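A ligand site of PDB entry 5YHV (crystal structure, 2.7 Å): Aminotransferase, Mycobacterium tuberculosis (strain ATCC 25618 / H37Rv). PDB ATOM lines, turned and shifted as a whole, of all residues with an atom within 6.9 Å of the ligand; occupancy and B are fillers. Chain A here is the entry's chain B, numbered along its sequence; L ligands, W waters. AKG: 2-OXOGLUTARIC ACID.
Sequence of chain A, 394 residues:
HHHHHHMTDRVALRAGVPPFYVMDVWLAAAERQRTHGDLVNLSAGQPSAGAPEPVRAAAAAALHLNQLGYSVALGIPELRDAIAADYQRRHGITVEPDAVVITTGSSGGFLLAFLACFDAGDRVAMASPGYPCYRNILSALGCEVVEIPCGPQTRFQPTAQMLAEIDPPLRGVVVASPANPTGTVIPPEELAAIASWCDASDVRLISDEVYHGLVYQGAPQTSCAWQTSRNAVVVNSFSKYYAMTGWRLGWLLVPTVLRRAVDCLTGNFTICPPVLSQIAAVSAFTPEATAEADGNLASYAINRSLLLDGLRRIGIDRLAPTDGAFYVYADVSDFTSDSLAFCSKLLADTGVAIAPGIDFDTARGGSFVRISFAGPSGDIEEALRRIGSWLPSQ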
ATOM      1  N   ILE A  83      -9.848   9.800  14.827  1.00  0.00           N
ATOM      2  CA  ILE A  83     -11.183  10.054  15.401  1.00  0.00           C
ATOM      3  C   ILE A  83     -11.690   8.824  16.166  1.00  0.00           C
ATOM      4  O   ILE A  83     -12.129   8.965  17.314  1.00  0.00           O
ATOM      5  CB  ILE A  83     -12.187  10.537  14.319  1.00  0.00           C
ATOM      6  CG1 ILE A  83     -11.849  11.961  13.891  1.00  0.00           C
ATOM      7  CG2 ILE A  83     -13.628  10.471  14.839  1.00  0.00           C
ATOM      8  CD1 ILE A  83     -12.419  12.387  12.558  1.00  0.00           C
ATOM      9  N   ASP A  86      -9.906   8.443  19.378  1.00  0.00           N
ATOM     10  CA  ASP A  86     -10.270   9.506  20.326  1.00  0.00           C
ATOM     11  C   ASP A  86     -11.486   9.126  21.174  1.00  0.00           C
ATOM     12  O   ASP A  86     -11.553   9.475  22.347  1.00  0.00           O
ATOM     13  CB  ASP A  86     -10.516  10.833  19.584  1.00  0.00           C
ATOM     14  CG  ASP A  86     -10.725  11.999  20.544  1.00  0.00           C
ATOM     15  OD1 ASP A  86      -9.781  12.350  21.291  1.00  0.00           O
ATOM     16  OD2 ASP A  86     -11.836  12.584  20.528  1.00  0.00           O
ATOM     17  N   TYR A  87     -12.433   8.409  20.556  1.00  0.00           N
ATOM     18  CA  TYR A  87     -13.613   7.887  21.263  1.00  0.00           C
ATOM     19  C   TYR A  87     -13.241   6.891  22.362  1.00  0.00           C
ATOM     20  O   TYR A  87     -13.879   6.866  23.421  1.00  0.00           O
ATOM     21  CB  TYR A  87     -14.600   7.237  20.275  1.00  0.00           C
ATOM     22  CG  TYR A  87     -15.487   8.232  19.569  1.00  0.00           C
ATOM     23  CD1 TYR A  87     -16.646   8.737  20.172  1.00  0.00           C
ATOM     24  CD2 TYR A  87     -15.175   8.677  18.272  1.00  0.00           C
ATOM     25  CE1 TYR A  87     -17.453   9.657  19.517  1.00  0.00           C
ATOM     26  CE2 TYR A  87     -15.978   9.591  17.608  1.00  0.00           C
ATOM     27  CZ  TYR A  87     -17.117  10.081  18.231  1.00  0.00           C
ATOM     28  OH  TYR A  87     -17.901  10.985  17.570  1.00  0.00           O
ATOM     29  N   ARG A  90     -10.524   8.962  25.173  1.00  0.00           N
ATOM     30  CA  ARG A  90     -11.152  10.003  25.989  1.00  0.00           C
ATOM     31  C   ARG A  90     -12.483   9.599  26.624  1.00  0.00           C
ATOM     32  O   ARG A  90     -12.812  10.075  27.711  1.00  0.00           O
ATOM     33  CB  ARG A  90     -11.289  11.301  25.195  1.00  0.00           C
ATOM     34  N   HIS A  91     -13.244   8.728  25.948  1.00  0.00           N
ATOM     35  CA  HIS A  91     -14.625   8.415  26.375  1.00  0.00           C
ATOM     36  C   HIS A  91     -14.952   6.918  26.520  1.00  0.00           C
ATOM     37  O   HIS A  91     -16.096   6.566  26.824  1.00  0.00           O
ATOM     38  CB  HIS A  91     -15.631   9.120  25.455  1.00  0.00           C
ATOM     39  CG  HIS A  91     -15.211  10.492  25.047  1.00  0.00           C
ATOM     40  ND1 HIS A  91     -15.295  11.569  25.904  1.00  0.00           N
ATOM     41  CD2 HIS A  91     -14.664  10.949  23.904  1.00  0.00           C
ATOM     42  CE1 HIS A  91     -14.829  12.644  25.289  1.00  0.00           C
ATOM     43  NE2 HIS A  91     -14.444  12.299  24.075  1.00  0.00           N
ATOM     44  N   GLY A  92     -13.946   6.067  26.311  1.00  0.00           N
ATOM     45  CA  GLY A  92     -14.052   4.628  26.557  1.00  0.00           C
ATOM     46  C   GLY A  92     -15.069   3.845  25.748  1.00  0.00           C
ATOM     47  O   GLY A  92     -15.582   2.823  26.211  1.00  0.00           O
ATOM     48  N   ILE A  93     -15.374   4.325  24.538  1.00  0.00           N
ATOM     49  CA  ILE A  93     -16.249   3.620  23.599  1.00  0.00           C
ATOM     50  C   ILE A  93     -15.432   3.147  22.395  1.00  0.00           C
ATOM     51  O   ILE A  93     -14.651   3.920  21.835  1.00  0.00           O
ATOM     52  CB  ILE A  93     -17.516   4.460  23.194  1.00  0.00           C
ATOM     53  CG1 ILE A  93     -18.323   3.797  22.067  1.00  0.00           C
ATOM     54  CG2 ILE A  93     -17.194   5.918  22.865  1.00  0.00           C
ATOM     55  N   GLU A 209     -23.618  16.245  18.196  1.00  0.00           N
ATOM     56  CA  GLU A 209     -22.652  16.212  19.292  1.00  0.00           C
ATOM     57  C   GLU A 209     -21.487  17.183  19.006  1.00  0.00           C
ATOM     58  O   GLU A 209     -20.367  17.013  19.506  1.00  0.00           O
ATOM     59  CB  GLU A 209     -22.168  14.771  19.508  1.00  0.00           C
ATOM     60  CG  GLU A 209     -23.301  13.796  19.876  1.00  0.00           C
ATOM     61  CD  GLU A 209     -22.814  12.387  20.161  1.00  0.00           C
ATOM     62  OE1 GLU A 209     -21.591  12.166  20.280  1.00  0.00           O
ATOM     63  OE2 GLU A 209     -23.689  11.481  20.267  1.00  0.00           O
ATOM     64  N   VAL A 210     -21.810  18.225  18.236  1.00  0.00           N
ATOM     65  CA  VAL A 210     -20.876  19.243  17.740  1.00  0.00           C
ATOM     66  C   VAL A 210     -20.150  20.004  18.865  1.00  0.00           C
ATOM     67  O   VAL A 210     -18.953  20.301  18.743  1.00  0.00           O
ATOM     68  CB  VAL A 210     -21.608  20.206  16.753  1.00  0.00           C
ATOM     69  CG1 VAL A 210     -20.790  21.433  16.382  1.00  0.00           C
ATOM     70  CG2 VAL A 210     -22.015  19.451  15.492  1.00  0.00           C
ATOM     71  N   HIS A 212     -19.562  18.921  21.976  1.00  0.00           N
ATOM     72  CA  HIS A 212     -18.847  18.032  22.887  1.00  0.00           C
ATOM     73  C   HIS A 212     -17.409  18.523  23.088  1.00  0.00           C
ATOM     74  O   HIS A 212     -16.758  18.979  22.146  1.00  0.00           O
ATOM     75  CB  HIS A 212     -18.822  16.608  22.333  1.00  0.00           C
ATOM     76  CG  HIS A 212     -20.071  15.820  22.605  1.00  0.00           C
ATOM     77  ND1 HIS A 212     -20.055  14.461  22.828  1.00  0.00           N
ATOM     78  CD2 HIS A 212     -21.367  16.200  22.692  1.00  0.00           C
ATOM     79  CE1 HIS A 212     -21.285  14.040  23.044  1.00  0.00           C
ATOM     80  NE2 HIS A 212     -22.101  15.073  22.957  1.00  0.00           N
ATOM     81  N   GLY A 213     -16.938  18.442  24.331  1.00  0.00           N
ATOM     82  CA  GLY A 213     -15.638  18.982  24.715  1.00  0.00           C
ATOM     83  C   GLY A 213     -15.730  20.370  25.321  1.00  0.00           C
ATOM     84  O   GLY A 213     -14.807  20.820  26.011  1.00  0.00           O
ATOM     85  N   GLN A 221     -23.100  15.450  32.653  1.00  0.00           N
ATOM     86  CA  GLN A 221     -22.047  14.921  31.800  1.00  0.00           C
ATOM     87  C   GLN A 221     -22.584  14.762  30.380  1.00  0.00           C
ATOM     88  O   GLN A 221     -23.779  14.554  30.173  1.00  0.00           O
ATOM     89  CB  GLN A 221     -21.492  13.599  32.364  1.00  0.00           C
ATOM     90  CG  GLN A 221     -20.568  13.752  33.554  1.00  0.00           C
ATOM     91  CD  GLN A 221     -20.199  12.429  34.199  1.00  0.00           C
ATOM     92  OE1 GLN A 221     -19.999  12.359  35.414  1.00  0.00           O
ATOM     93  NE2 GLN A 221     -20.122  11.374  33.402  1.00  0.00           N
ATOM     94  N   THR A 222     -21.681  14.850  29.410  1.00  0.00           N
ATOM     95  CA  THR A 222     -22.068  14.619  28.027  1.00  0.00           C
ATOM     96  C   THR A 222     -21.827  13.140  27.723  1.00  0.00           C
ATOM     97  O   THR A 222     -20.985  12.489  28.349  1.00  0.00           O
ATOM     98  CB  THR A 222     -21.333  15.512  27.016  1.00  0.00           C
ATOM     99  OG1 THR A 222     -19.916  15.323  27.152  1.00  0.00           O
ATOM    100  CG2 THR A 222     -21.744  16.979  27.141  1.00  0.00           C
ATOM    101  N   SER A 223     -22.579  12.641  26.758  1.00  0.00           N
ATOM    102  CA  SER A 223     -22.492  11.238  26.346  1.00  0.00           C
ATOM    103  C   SER A 223     -22.760  11.096  24.853  1.00  0.00           C
ATOM    104  O   SER A 223     -23.477  11.902  24.254  1.00  0.00           O
ATOM    105  CB  SER A 223     -23.456  10.368  27.153  1.00  0.00           C
ATOM    106  OG  SER A 223     -24.769  10.901  27.144  1.00  0.00           O
ATOM    107  N   CYS A 224     -22.139  10.079  24.254  1.00  0.00           N
ATOM    108  CA  CYS A 224     -22.356   9.755  22.866  1.00  0.00           C
ATOM    109  C   CYS A 224     -23.567   8.839  22.749  1.00  0.00           C
ATOM    110  O   CYS A 224     -23.765   7.939  23.580  1.00  0.00           O
ATOM    111  CB  CYS A 224     -21.128   9.089  22.254  1.00  0.00           C
ATOM    112  SG  CYS A 224     -21.323   8.708  20.497  1.00  0.00           S
ATOM    113  N   ALA A 225     -24.379   9.060  21.706  1.00  0.00           N
ATOM    114  CA  ALA A 225     -25.538   8.224  21.407  1.00  0.00           C
ATOM    115  C   ALA A 225     -25.167   6.754  21.228  1.00  0.00           C
ATOM    116  O   ALA A 225     -25.971   5.868  21.560  1.00  0.00           O
ATOM    117  CB  ALA A 225     -26.271   8.736  20.178  1.00  0.00           C
ATOM    118  N   GLN A 227     -23.182   5.052  22.959  1.00  0.00           N
ATOM    119  CA  GLN A 227     -23.084   4.369  24.249  1.00  0.00           C
ATOM    120  C   GLN A 227     -24.322   3.503  24.506  1.00  0.00           C
ATOM    121  O   GLN A 227     -24.230   2.468  25.162  1.00  0.00           O
ATOM    122  CB  GLN A 227     -22.875   5.363  25.394  1.00  0.00           C
ATOM    123  CG  GLN A 227     -21.494   5.994  25.400  1.00  0.00           C
ATOM    124  CD  GLN A 227     -21.288   7.003  26.520  1.00  0.00           C
ATOM    125  OE1 GLN A 227     -20.885   8.144  26.265  1.00  0.00           O
ATOM    126  NE2 GLN A 227     -21.559   6.601  27.750  1.00  0.00           N
ATOM    127  N   VAL A 234     -24.442   9.858  14.523  1.00  0.00           N
ATOM    128  CA  VAL A 234     -23.731  10.857  15.318  1.00  0.00           C
ATOM    129  C   VAL A 234     -23.134  11.894  14.379  1.00  0.00           C
ATOM    130  O   VAL A 234     -22.453  11.544  13.409  1.00  0.00           O
ATOM    131  CB  VAL A 234     -22.634  10.217  16.200  1.00  0.00           C
ATOM    132  CG1 VAL A 234     -21.825  11.267  16.959  1.00  0.00           C
ATOM    133  CG2 VAL A 234     -23.225   9.197  17.155  1.00  0.00           C
ATOM    134  N   VAL A 235     -23.406  13.163  14.657  1.00  0.00           N
ATOM    135  CA  VAL A 235     -22.858  14.278  13.889  1.00  0.00           C
ATOM    136  C   VAL A 235     -21.930  15.065  14.802  1.00  0.00           C
ATOM    137  O   VAL A 235     -22.306  15.425  15.931  1.00  0.00           O
ATOM    138  CB  VAL A 235     -23.963  15.180  13.294  1.00  0.00           C
ATOM    139  CG1 VAL A 235     -23.376  16.177  12.315  1.00  0.00           C
ATOM    140  CG2 VAL A 235     -25.049  14.349  12.612  1.00  0.00           C
ATOM    141  N   ASN A 236     -20.710  15.313  14.331  1.00  0.00           N
ATOM    142  CA  ASN A 236     -19.718  16.079  15.075  1.00  0.00           C
ATOM    143  C   ASN A 236     -18.855  16.911  14.123  1.00  0.00           C
ATOM    144  O   ASN A 236     -18.916  16.731  12.903  1.00  0.00           O
ATOM    145  CB  ASN A 236     -18.861  15.156  15.939  1.00  0.00           C
ATOM    146  CG  ASN A 236     -18.426  15.796  17.259  1.00  0.00           C
ATOM    147  OD1 ASN A 236     -18.124  16.995  17.326  1.00  0.00           O
ATOM    148  ND2 ASN A 236     -18.401  14.992  18.320  1.00  0.00           N
ATOM    149  N   SER A 237     -18.067  17.819  14.677  1.00  0.00           N
ATOM    150  CA  SER A 237     -17.309  18.787  13.895  1.00  0.00           C
ATOM    151  C   SER A 237     -15.982  19.187  14.540  1.00  0.00           C
ATOM    152  O   SER A 237     -15.784  18.995  15.740  1.00  0.00           O
ATOM    153  CB  SER A 237     -18.158  20.043  13.655  1.00  0.00           C
ATOM    154  OG  SER A 237     -17.460  20.963  12.831  1.00  0.00           O
ATOM    155  N   TYR A 241     -15.029  22.877  19.172  1.00  0.00           N
ATOM    156  CA  TYR A 241     -14.062  22.497  20.186  1.00  0.00           C
ATOM    157  C   TYR A 241     -12.632  22.758  19.714  1.00  0.00           C
ATOM    158  O   TYR A 241     -11.824  23.303  20.456  1.00  0.00           O
ATOM    159  CB  TYR A 241     -14.246  21.047  20.646  1.00  0.00           C
ATOM    160  CG  TYR A 241     -13.176  20.580  21.611  1.00  0.00           C
ATOM    161  CD1 TYR A 241     -13.103  21.099  22.911  1.00  0.00           C
ATOM    162  CD2 TYR A 241     -12.231  19.623  21.219  1.00  0.00           C
ATOM    163  CE1 TYR A 241     -12.114  20.678  23.794  1.00  0.00           C
ATOM    164  CE2 TYR A 241     -11.247  19.199  22.089  1.00  0.00           C
ATOM    165  CZ  TYR A 241     -11.191  19.723  23.379  1.00  0.00           C
ATOM    166  OH  TYR A 241     -10.215  19.301  24.245  1.00  0.00           O
ATOM    167  N   TRP A 251     -17.206  15.107  11.010  1.00  0.00           N
ATOM    168  CA  TRP A 251     -17.387  13.675  10.799  1.00  0.00           C
ATOM    169  C   TRP A 251     -18.742  13.135  11.236  1.00  0.00           C
ATOM    170  O   TRP A 251     -19.451  13.775  12.016  1.00  0.00           O
ATOM    171  CB  TRP A 251     -16.241  12.868  11.431  1.00  0.00           C
ATOM    172  CG  TRP A 251     -16.298  12.775  12.926  1.00  0.00           C
ATOM    173  CD1 TRP A 251     -16.914  11.806  13.675  1.00  0.00           C
ATOM    174  CD2 TRP A 251     -15.706  13.676  13.865  1.00  0.00           C
ATOM    175  NE1 TRP A 251     -16.742  12.044  15.016  1.00  0.00           N
ATOM    176  CE2 TRP A 251     -16.002  13.194  15.158  1.00  0.00           C
ATOM    177  CE3 TRP A 251     -14.946  14.858  13.740  1.00  0.00           C
ATOM    178  CZ2 TRP A 251     -15.561  13.835  16.334  1.00  0.00           C
ATOM    179  CZ3 TRP A 251     -14.514  15.502  14.911  1.00  0.00           C
ATOM    180  CH2 TRP A 251     -14.831  14.983  16.183  1.00  0.00           C
ATOM    181  N   LEU A 253     -20.533   9.351  12.662  1.00  0.00           N
ATOM    182  CA  LEU A 253     -20.520   7.924  12.975  1.00  0.00           C
ATOM    183  C   LEU A 253     -21.750   7.323  12.297  1.00  0.00           C
ATOM    184  O   LEU A 253     -22.884   7.622  12.670  1.00  0.00           O
ATOM    185  CB  LEU A 253     -20.507   7.661  14.495  1.00  0.00           C
ATOM    186  CG  LEU A 253     -19.391   8.253  15.369  1.00  0.00           C
ATOM    187  CD1 LEU A 253     -19.568   7.784  16.807  1.00  0.00           C
ATOM    188  CD2 LEU A 253     -17.992   7.920  14.868  1.00  0.00           C
ATOM    189  N   PHE A 285      -5.367  15.869  17.395  1.00  0.00           N
ATOM    190  CA  PHE A 285      -5.390  14.855  18.437  1.00  0.00           C
ATOM    191  C   PHE A 285      -4.052  14.697  19.175  1.00  0.00           C
ATOM    192  O   PHE A 285      -3.822  13.710  19.866  1.00  0.00           O
ATOM    193  CB  PHE A 285      -5.931  13.533  17.861  1.00  0.00           C
ATOM    194  CG  PHE A 285      -7.310  13.658  17.289  1.00  0.00           C
ATOM    195  CD1 PHE A 285      -8.432  13.661  18.126  1.00  0.00           C
ATOM    196  CD2 PHE A 285      -7.497  13.807  15.915  1.00  0.00           C
ATOM    197  CE1 PHE A 285      -9.713  13.800  17.596  1.00  0.00           C
ATOM    198  CE2 PHE A 285      -8.778  13.945  15.385  1.00  0.00           C
ATOM    199  CZ  PHE A 285      -9.893  13.932  16.224  1.00  0.00           C
HETATM  200  C1  AKG L   1     -16.295  13.190  20.835  1.00  0.00           C
HETATM  201  O1  AKG L   1     -15.350  12.369  20.815  1.00  0.00           O
HETATM  202  O2  AKG L   1     -16.231  14.297  20.254  1.00  0.00           O
HETATM  203  C2  AKG L   1     -17.525  12.874  21.563  1.00  0.00           C
HETATM  204  O5  AKG L   1     -18.566  12.758  20.943  1.00  0.00           O
HETATM  205  C3  AKG L   1     -17.481  12.723  23.065  1.00  0.00           C
HETATM  206  C4  AKG L   1     -18.202  11.454  23.495  1.00  0.00           C
HETATM  207  C5  AKG L   1     -18.564  11.432  24.968  1.00  0.00           C
HETATM  208  O3  AKG L   1     -18.533  10.321  25.552  1.00  0.00           O
HETATM  209  O4  AKG L   1     -18.898  12.486  25.554  1.00  0.00           O
HETATM  210  O   HOH W   1     -13.496  15.670  20.632  1.00  0.00           O
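ND1 of His 212 sits at hydrogen-bond distance from O5 of the ligand. O4 of the ligand sits at hydrogen-bond distance from OG1 of Thr 222 (3.4 Å). NE2 of His 91 lies close to O1 of the ligand, at 3.4 Å. The side-chain amide nitrogen of Asn 236 is in hydrogen-bond range of an oxygen (O2) of the ligand. The side-chain amide oxygen of Gln 227 lies close to an oxygen (O3) of the ligand (3.3 Å).
O of Val 235 lies within hydrogen-bond range of N of Glu 209, 2.7 Å away. The backbone NH (N) of Gly 92 sits at hydrogen-bond distance from the backbone carbonyl oxygen (O) of Tyr 87 (3.0 Å). O of Glu 209 sits at hydrogen-bond distance from ND2 of Asn 236 (3.1 Å). The side-chain sulfur of Cys 224 lies within hydrogen-bond range of the side-chain carboxylate of Glu 209. The backbone carbonyl oxygen (O) of Tyr 87 sits at hydrogen-bond distance from the backbone NH (N) of Ile 93, at 3.2 Å. The side-chain hydroxyl (OH) of Tyr 87 is in hydrogen-bond range of the indole nitrogen (NE1) of Trp 251 (3.0 Å). N of Trp 251 is in hydrogen-bond range of O of Asn 236. N of Cys 224 sits at hydrogen-bond distance from OE1 of Gln 227, 3.1 Å away.
The side-chain carboxylate (OE1) of Glu 209 lies close to an oxygen (O5) of the ligand, 3.2 Å away. Asp 86 touches the ligand (OD2 to O1, 3.5 Å). Tyr 87 touches the ligand (CE1 to O5, 3.6 Å). N of Ser 223 touches O4 of the ligand, at 3.9 Å. Cys 224 touches the ligand. Within 4 Å of the ligand: Asp 86, Tyr 87, His 91, Glu 209, His 212, Thr 222, Ser 223, Cys 224, Gln 227 and Asn 236. The nearest printed residue that does not touch the ligand is Trp 251 (4.004 Å).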
